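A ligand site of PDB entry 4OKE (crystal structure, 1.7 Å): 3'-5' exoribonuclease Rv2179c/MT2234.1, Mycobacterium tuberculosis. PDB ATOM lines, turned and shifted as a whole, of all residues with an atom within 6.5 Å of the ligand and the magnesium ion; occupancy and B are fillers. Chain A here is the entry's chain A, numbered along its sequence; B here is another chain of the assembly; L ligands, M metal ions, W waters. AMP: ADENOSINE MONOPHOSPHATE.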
ATOM      1  N   TYR A   5     -16.375   9.169   9.802  1.00  0.00           N
ATOM      2  CA  TYR A   5     -14.923   9.384  10.085  1.00  0.00           C
ATOM      3  C   TYR A   5     -14.070   8.616   9.085  1.00  0.00           C
ATOM      4  O   TYR A   5     -14.538   7.663   8.418  1.00  0.00           O
ATOM      5  CB  TYR A   5     -14.594   9.091  11.561  1.00  0.00           C
ATOM      6  CG  TYR A   5     -14.629   7.637  11.947  1.00  0.00           C
ATOM      7  CD1 TYR A   5     -15.839   6.965  12.115  1.00  0.00           C
ATOM      8  CD2 TYR A   5     -13.430   6.909  12.086  1.00  0.00           C
ATOM      9  CE1 TYR A   5     -15.821   5.601  12.445  1.00  0.00           C
ATOM     10  CE2 TYR A   5     -13.407   5.596  12.411  1.00  0.00           C
ATOM     11  CZ  TYR A   5     -14.598   4.939  12.579  1.00  0.00           C
ATOM     12  OH  TYR A   5     -14.587   3.646  12.913  1.00  0.00           O
ATOM     13  N   ASP A   6     -12.790   8.963   9.057  1.00  0.00           N
ATOM     14  CA  ASP A   6     -11.795   8.263   8.279  1.00  0.00           C
ATOM     15  C   ASP A   6     -10.490   8.398   9.046  1.00  0.00           C
ATOM     16  O   ASP A   6     -10.326   9.321   9.778  1.00  0.00           O
ATOM     17  CB  ASP A   6     -11.633   8.859   6.898  1.00  0.00           C
ATOM     18  CG  ASP A   6     -10.586   8.106   6.056  1.00  0.00           C
ATOM     19  OD1 ASP A   6     -10.877   6.964   5.771  1.00  0.00           O
ATOM     20  OD2 ASP A   6      -9.504   8.679   5.733  1.00  0.00           O
ATOM     21  N   THR A   7      -9.632   7.421   8.803  1.00  0.00           N
ATOM     22  CA  THR A   7      -8.314   7.492   9.466  1.00  0.00           C
ATOM     23  C   THR A   7      -7.231   7.191   8.476  1.00  0.00           C
ATOM     24  O   THR A   7      -7.481   6.486   7.502  1.00  0.00           O
ATOM     25  CB  THR A   7      -8.176   6.464  10.631  1.00  0.00           C
ATOM     26  OG1 THR A   7      -8.240   5.090  10.136  1.00  0.00           O
ATOM     27  CG2 THR A   7      -9.288   6.691  11.708  1.00  0.00           C
ATOM     28  N   GLU A   8      -6.036   7.697   8.679  1.00  0.00           N
ATOM     29  CA  GLU A   8      -4.863   7.280   7.908  1.00  0.00           C
ATOM     30  C   GLU A   8      -3.956   6.617   8.904  1.00  0.00           C
ATOM     31  O   GLU A   8      -3.967   7.002  10.094  1.00  0.00           O
ATOM     32  CB  GLU A   8      -4.157   8.447   7.212  1.00  0.00           C
ATOM     33  CG  GLU A   8      -5.081   9.193   6.236  1.00  0.00           C
ATOM     34  CD  GLU A   8      -5.528   8.319   5.055  1.00  0.00           C
ATOM     35  OE1 GLU A   8      -4.792   7.465   4.618  1.00  0.00           O
ATOM     36  OE2 GLU A   8      -6.658   8.517   4.576  1.00  0.00           O
ATOM     37  N   PHE A   9      -3.193   5.637   8.429  1.00  0.00           N
ATOM     38  CA  PHE A   9      -2.398   4.792   9.356  1.00  0.00           C
ATOM     39  C   PHE A   9      -1.299   4.051   8.640  1.00  0.00           C
ATOM     40  O   PHE A   9      -1.260   4.051   7.378  1.00  0.00           O
ATOM     41  CB  PHE A   9      -3.315   3.846  10.189  1.00  0.00           C
ATOM     42  CG  PHE A   9      -4.275   3.060   9.333  1.00  0.00           C
ATOM     43  CD1 PHE A   9      -3.804   2.021   8.514  1.00  0.00           C
ATOM     44  CD2 PHE A   9      -5.654   3.374   9.341  1.00  0.00           C
ATOM     45  CE1 PHE A   9      -4.661   1.290   7.691  1.00  0.00           C
ATOM     46  CE2 PHE A   9      -6.527   2.642   8.534  1.00  0.00           C
ATOM     47  CZ  PHE A   9      -6.044   1.607   7.733  1.00  0.00           C
ATOM     48  N   ILE A  10      -0.346   3.470   9.422  1.00  0.00           N
ATOM     49  CA  ILE A  10       0.694   2.619   8.875  1.00  0.00           C
ATOM     50  C   ILE A  10       0.383   1.266   9.497  1.00  0.00           C
ATOM     51  O   ILE A  10       0.374   1.130  10.694  1.00  0.00           O
ATOM     52  CB  ILE A  10       2.118   3.079   9.299  1.00  0.00           C
ATOM     53  CG1 ILE A  10       2.480   4.394   8.599  1.00  0.00           C
ATOM     54  CG2 ILE A  10       3.169   1.968   8.867  1.00  0.00           C
ATOM     55  CD1 ILE A  10       3.633   5.144   9.286  1.00  0.00           C
ATOM     56  N   GLU A  11      -0.007   0.319   8.662  1.00  0.00           N
ATOM     57  CA  GLU A  11      -0.448  -0.968   9.118  1.00  0.00           C
ATOM     58  C   GLU A  11       0.447  -2.050   8.499  1.00  0.00           C
ATOM     59  O   GLU A  11       0.777  -1.980   7.399  1.00  0.00           O
ATOM     60  CB  GLU A  11      -1.915  -1.132   8.729  1.00  0.00           C
ATOM     61  CG  GLU A  11      -2.510  -2.367   9.111  1.00  0.00           C
ATOM     62  CD  GLU A  11      -2.256  -3.503   8.152  1.00  0.00           C
ATOM     63  OE1 GLU A  11      -2.186  -3.314   6.961  1.00  0.00           O
ATOM     64  OE2 GLU A  11      -2.155  -4.539   8.655  1.00  0.00           O
ATOM     65  N   ILE A  19      -1.935   7.693  11.985  1.00  0.00           N
ATOM     66  CA  ILE A  19      -1.405   8.952  11.471  1.00  0.00           C
ATOM     67  C   ILE A  19      -2.399  10.099  11.741  1.00  0.00           C
ATOM     68  O   ILE A  19      -2.058  11.101  12.343  1.00  0.00           O
ATOM     69  CB  ILE A  19      -1.084   8.838   9.929  1.00  0.00           C
ATOM     70  CG1 ILE A  19       0.167   7.954   9.710  1.00  0.00           C
ATOM     71  CG2 ILE A  19      -0.894  10.272   9.292  1.00  0.00           C
ATOM     72  CD1 ILE A  19       0.314   7.489   8.280  1.00  0.00           C
ATOM     73  N   TRP A  46       3.468   3.887  -0.658  1.00  0.00           N
ATOM     74  CA  TRP A  46       2.127   4.404  -0.878  1.00  0.00           C
ATOM     75  C   TRP A  46       1.779   5.504   0.157  1.00  0.00           C
ATOM     76  O   TRP A  46       1.281   6.596  -0.205  1.00  0.00           O
ATOM     77  CB  TRP A  46       1.120   3.281  -0.829  1.00  0.00           C
ATOM     78  CG  TRP A  46      -0.246   3.725  -1.277  1.00  0.00           C
ATOM     79  CD1 TRP A  46      -0.751   3.665  -2.553  1.00  0.00           C
ATOM     80  CD2 TRP A  46      -1.285   4.293  -0.461  1.00  0.00           C
ATOM     81  NE1 TRP A  46      -2.044   4.156  -2.584  1.00  0.00           N
ATOM     82  CE2 TRP A  46      -2.396   4.549  -1.312  1.00  0.00           C
ATOM     83  CE3 TRP A  46      -1.397   4.598   0.908  1.00  0.00           C
ATOM     84  CZ2 TRP A  46      -3.584   5.103  -0.837  1.00  0.00           C
ATOM     85  CZ3 TRP A  46      -2.556   5.148   1.375  1.00  0.00           C
ATOM     86  CH2 TRP A  46      -3.661   5.386   0.503  1.00  0.00           C
ATOM     87  N   VAL A  47       2.039   5.215   1.421  1.00  0.00           N
ATOM     88  CA  VAL A  47       1.783   6.193   2.490  1.00  0.00           C
ATOM     89  C   VAL A  47       2.664   7.447   2.362  1.00  0.00           C
ATOM     90  O   VAL A  47       2.175   8.584   2.498  1.00  0.00           O
ATOM     91  CB  VAL A  47       1.876   5.555   3.942  1.00  0.00           C
ATOM     92  CG1 VAL A  47       1.923   6.681   5.032  1.00  0.00           C
ATOM     93  CG2 VAL A  47       0.694   4.653   4.213  1.00  0.00           C
ATOM     94  N   VAL A  51      -0.239  10.000   1.534  1.00  0.00           N
ATOM     95  CA  VAL A  51      -0.692  10.462   2.835  1.00  0.00           C
ATOM     96  C   VAL A  51       0.195  11.546   3.460  1.00  0.00           C
ATOM     97  O   VAL A  51      -0.311  12.628   3.822  1.00  0.00           O
ATOM     98  CB  VAL A  51      -0.858   9.216   3.810  1.00  0.00           C
ATOM     99  CG1 VAL A  51      -1.306   9.645   5.208  1.00  0.00           C
ATOM    100  CG2 VAL A  51      -1.873   8.163   3.174  1.00  0.00           C
ATOM    101  N   TRP A  90     -16.548   4.414   5.475  1.00  0.00           N
ATOM    102  CA  TRP A  90     -16.576   3.603   4.238  1.00  0.00           C
ATOM    103  C   TRP A  90     -15.405   2.563   4.289  1.00  0.00           C
ATOM    104  O   TRP A  90     -14.248   2.962   4.139  1.00  0.00           O
ATOM    105  CB  TRP A  90     -16.264   4.536   3.076  1.00  0.00           C
ATOM    106  CG  TRP A  90     -16.398   3.939   1.759  1.00  0.00           C
ATOM    107  CD1 TRP A  90     -15.446   3.296   1.036  1.00  0.00           C
ATOM    108  CD2 TRP A  90     -17.557   4.026   0.920  1.00  0.00           C
ATOM    109  NE1 TRP A  90     -15.951   2.889  -0.146  1.00  0.00           N
ATOM    110  CE2 TRP A  90     -17.256   3.318  -0.259  1.00  0.00           C
ATOM    111  CE3 TRP A  90     -18.838   4.599   1.069  1.00  0.00           C
ATOM    112  CZ2 TRP A  90     -18.183   3.178  -1.302  1.00  0.00           C
ATOM    113  CZ3 TRP A  90     -19.757   4.456   0.022  1.00  0.00           C
ATOM    114  CH2 TRP A  90     -19.408   3.762  -1.148  1.00  0.00           C
ATOM    115  N   VAL A  91     -15.711   1.274   4.427  1.00  0.00           N
ATOM    116  CA  VAL A  91     -14.708   0.143   4.354  1.00  0.00           C
ATOM    117  C   VAL A  91     -13.920   0.424   5.631  1.00  0.00           C
ATOM    118  O   VAL A  91     -12.737   0.867   5.600  1.00  0.00           O
ATOM    119  CB  VAL A  91     -13.810   0.223   3.090  1.00  0.00           C
ATOM    120  CG1 VAL A  91     -12.737  -0.884   3.080  1.00  0.00           C
ATOM    121  CG2 VAL A  91     -14.686   0.026   1.813  1.00  0.00           C
ATOM    122  N   ASP A  95     -10.398   1.237  10.345  1.00  0.00           N
ATOM    123  CA  ASP A  95     -10.683   2.535  10.963  1.00  0.00           C
ATOM    124  C   ASP A  95     -11.271   2.378  12.314  1.00  0.00           C
ATOM    125  O   ASP A  95     -10.906   3.158  13.221  1.00  0.00           O
ATOM    126  CB  ASP A  95     -11.651   3.362  10.067  1.00  0.00           C
ATOM    127  CG  ASP A  95     -11.041   3.631   8.719  1.00  0.00           C
ATOM    128  OD1 ASP A  95     -10.212   4.505   8.596  1.00  0.00           O
ATOM    129  OD2 ASP A  95     -11.377   2.920   7.749  1.00  0.00           O
ATOM    130  N   VAL A 139      -8.231  13.265  -1.665  1.00  0.00           N
ATOM    131  CA  VAL A 139      -8.473  12.085  -0.891  1.00  0.00           C
ATOM    132  C   VAL A 139      -7.098  11.699  -0.320  1.00  0.00           C
ATOM    133  O   VAL A 139      -6.018  12.037  -0.887  1.00  0.00           O
ATOM    134  CB  VAL A 139      -9.191  10.963  -1.729  1.00  0.00           C
ATOM    135  CG1 VAL A 139      -8.893   9.593  -1.201  1.00  0.00           C
ATOM    136  CG2 VAL A 139     -10.708  11.193  -1.691  1.00  0.00           C
ATOM    137  N   HIS A 140      -7.199  11.041   0.806  1.00  0.00           N
ATOM    138  CA  HIS A 140      -6.134  10.598   1.666  1.00  0.00           C
ATOM    139  C   HIS A 140      -5.787  11.656   2.688  1.00  0.00           C
ATOM    140  O   HIS A 140      -4.925  11.472   3.501  1.00  0.00           O
ATOM    141  CB  HIS A 140      -4.978  10.050   0.872  1.00  0.00           C
ATOM    142  CG  HIS A 140      -5.401   9.044  -0.129  1.00  0.00           C
ATOM    143  ND1 HIS A 140      -6.220   7.998   0.176  1.00  0.00           N
ATOM    144  CD2 HIS A 140      -5.142   8.938  -1.445  1.00  0.00           C
ATOM    145  CE1 HIS A 140      -6.438   7.281  -0.904  1.00  0.00           C
ATOM    146  NE2 HIS A 140      -5.794   7.833  -1.899  1.00  0.00           N
ATOM    147  N   ASP A 141      -6.562  12.728   2.668  1.00  0.00           N
ATOM    148  CA  ASP A 141      -6.519  13.712   3.766  1.00  0.00           C
ATOM    149  C   ASP A 141      -7.728  13.287   4.597  1.00  0.00           C
ATOM    150  O   ASP A 141      -8.834  13.293   4.082  1.00  0.00           O
ATOM    151  CB  ASP A 141      -6.756  15.143   3.238  1.00  0.00           C
ATOM    152  CG  ASP A 141      -6.940  16.143   4.353  1.00  0.00           C
ATOM    153  OD1 ASP A 141      -7.796  15.926   5.251  1.00  0.00           O
ATOM    154  OD2 ASP A 141      -6.220  17.162   4.344  1.00  0.00           O
ATOM    155  N   ASP A 145     -11.687  13.102   3.414  1.00  0.00           N
ATOM    156  CA  ASP A 145     -12.357  11.804   3.258  1.00  0.00           C
ATOM    157  C   ASP A 145     -13.611  11.723   4.131  1.00  0.00           C
ATOM    158  O   ASP A 145     -14.713  11.376   3.658  1.00  0.00           O
ATOM    159  CB  ASP A 145     -11.373  10.695   3.631  1.00  0.00           C
ATOM    160  CG  ASP A 145     -10.199  10.559   2.662  1.00  0.00           C
ATOM    161  OD1 ASP A 145     -10.151  11.295   1.645  1.00  0.00           O
ATOM    162  OD2 ASP A 145      -9.271   9.713   2.943  1.00  0.00           O
ATOM    163  N   GLN A 149     -17.593  11.228   3.042  1.00  0.00           N
ATOM    164  CA  GLN A 149     -18.525  10.155   3.466  1.00  0.00           C
ATOM    165  C   GLN A 149     -19.886  10.648   3.895  1.00  0.00           C
ATOM    166  O   GLN A 149     -20.926  10.010   3.587  1.00  0.00           O
ATOM    167  CB  GLN A 149     -17.926   9.210   4.547  1.00  0.00           C
ATOM    168  CG  GLN A 149     -16.471   8.824   4.315  1.00  0.00           C
ATOM    169  CD  GLN A 149     -16.122   8.106   3.013  1.00  0.00           C
ATOM    170  OE1 GLN A 149     -14.907   7.985   2.729  1.00  0.00           O
ATOM    171  NE2 GLN A 149     -17.080   7.626   2.241  1.00  0.00           N
ATOM    172  N   MET B 106      -2.783  -5.512   4.993  1.00  0.00           N
ATOM    173  CA  MET B 106      -4.046  -5.671   4.210  1.00  0.00           C
ATOM    174  C   MET B 106      -3.834  -5.939   2.690  1.00  0.00           C
ATOM    175  O   MET B 106      -4.586  -6.696   2.050  1.00  0.00           O
ATOM    176  CB  MET B 106      -4.970  -4.452   4.444  1.00  0.00           C
ATOM    177  CG  MET B 106      -4.190  -3.123   4.322  1.00  0.00           C
ATOM    178  SD  MET B 106      -5.037  -1.531   4.707  1.00  0.00           S
ATOM    179  CE  MET B 106      -6.093  -1.873   6.029  1.00  0.00           C
ATOM    180  N   THR B 107      -2.796  -5.318   2.171  1.00  0.00           N
ATOM    181  CA  THR B 107      -2.120  -5.602   0.921  1.00  0.00           C
ATOM    182  C   THR B 107      -2.067  -7.046   0.470  1.00  0.00           C
ATOM    183  O   THR B 107      -2.254  -7.329  -0.734  1.00  0.00           O
ATOM    184  CB  THR B 107      -0.665  -5.175   1.125  1.00  0.00           C
ATOM    185  OG1 THR B 107      -0.515  -3.921   0.503  1.00  0.00           O
ATOM    186  CG2 THR B 107       0.381  -6.203   0.561  1.00  0.00           C
HETATM  187  P   AMP L   1      -7.697   5.737   2.885  1.00  0.00           P
HETATM  188  O1P AMP L   1      -6.933   7.011   2.644  1.00  0.00           O
HETATM  189  O2P AMP L   1      -8.749   5.982   3.884  1.00  0.00           O
HETATM  190  O3P AMP L   1      -8.069   5.187   1.545  1.00  0.00           O
HETATM  191  O5' AMP L   1      -6.776   4.528   3.454  1.00  0.00           O
HETATM  192  C5' AMP L   1      -6.406   4.466   4.881  1.00  0.00           C
HETATM  193  C4' AMP L   1      -5.124   3.721   5.111  1.00  0.00           C
HETATM  194  O4' AMP L   1      -5.124   2.438   4.410  1.00  0.00           O
HETATM  195  C3' AMP L   1      -3.913   4.411   4.527  1.00  0.00           C
HETATM  196  O3' AMP L   1      -3.465   5.446   5.423  1.00  0.00           O
HETATM  197  C2' AMP L   1      -2.922   3.285   4.237  1.00  0.00           C
HETATM  198  O2' AMP L   1      -2.277   2.796   5.398  1.00  0.00           O
HETATM  199  C1' AMP L   1      -3.878   2.181   3.717  1.00  0.00           C
HETATM  200  N9  AMP L   1      -4.108   2.091   2.239  1.00  0.00           N
HETATM  201  C8  AMP L   1      -5.250   2.528   1.547  1.00  0.00           C
HETATM  202  N7  AMP L   1      -5.232   2.320   0.222  1.00  0.00           N
HETATM  203  C5  AMP L   1      -3.997   1.694   0.051  1.00  0.00           C
HETATM  204  C6  AMP L   1      -3.329   1.215  -1.115  1.00  0.00           C
HETATM  205  N6  AMP L   1      -3.892   1.293  -2.335  1.00  0.00           N
HETATM  206  N1  AMP L   1      -2.069   0.661  -0.970  1.00  0.00           N
HETATM  207  C2  AMP L   1      -1.521   0.582   0.267  1.00  0.00           C
HETATM  208  N3  AMP L   1      -2.047   0.994   1.431  1.00  0.00           N
HETATM  209  C4  AMP L   1      -3.297   1.543   1.264  1.00  0.00           C
HETATM  210 MG    MG M   1     -10.388   5.068   4.646  1.00  0.00          MG
HETATM  211  O   HOH W   1      -9.227   4.902   6.339  1.00  0.00           O
HETATM  212  O   HOH W   2     -11.789   5.701   3.230  1.00  0.00           O
HETATM  213  O   HOH W   3      -9.756   3.135   3.627  1.00  0.00           O
HETATM  214  O   HOH W   4      -0.333   1.159   5.905  1.00  0.00           O
HETATM  215  O   HOH W   5     -10.291   7.309   0.439  1.00  0.00           O
HETATM  216  O   HOH W   6     -11.835   4.114   5.624  1.00  0.00           O
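OE1 of Glu 8 is in hydrogen-bond range of O3' of the ligand (2.5 Å). The backbone NH (N) of Phe 9 sits at hydrogen-bond distance from an oxygen (O3') of the ligand, 3.0 Å away. O2' of the ligand sits at hydrogen-bond distance from O of Phe 9, 2.6 Å away. A ring nitrogen (ND1) of His 140 lies within hydrogen-bond range of an oxygen (O1P) of the ligand (2.8 Å).
The backbone carbonyl oxygen (O) of Glu 8 sits at hydrogen-bond distance from the backbone NH (N) of Ile 19 (2.9 Å). The side-chain carboxylate (OD1) of Asp 145 is in hydrogen-bond range of the backbone NH (N) of His 140 (3.1 Å). OG1 of Thr 7 sits at hydrogen-bond distance from OD1 of Asp 95 (2.6 Å). The backbone NH (N) of Met 106 of chain B lies within hydrogen-bond range of the side-chain carboxylate (OE1) of Glu 11, at 3.0 Å.
A nitrogen (N6) of the ligand sits close to the indole nitrogen (NE1) of Trp 46. Merely in contact with the ligand: Thr 7 (3.5 Å), Asp 145 (3.6 Å), Val 47 (3.7 Å), Val 51 (3.9 Å) and Met 106 of chain B (3.98 Å). Hydrophobic or aromatic side chains within 4 Å of the ligand: Phe 9, Trp 46, Val 47, Val 51, His 140 and Met 106 of chain B. Of the 21 residues printed, 10 come within 4 Å of the ligand.
Merely in contact with the magnesium ion: Asp 95 (3.9 Å). Two residues have an atom within 4 Å of the magnesium ion: Asp 6 and Asp 95.
The magnesium ion is bound by water W6 (2.0 Å), an oxygen (O2P) of the ligand (2.0 Å), water W1 (2.1 Å), water W2 (2.1 Å), the side-chain carboxylate of Asp 6 (2.3 Å) and water W3 (2.3 Å).
Water W1 lies within hydrogen-bond range of OD1 of Asp 95 (2.5 Å) and O of Thr 7 (2.6 Å). Water W4 lies within hydrogen-bond range of O2' of the ligand, N of Glu 11 and O of Phe 9.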
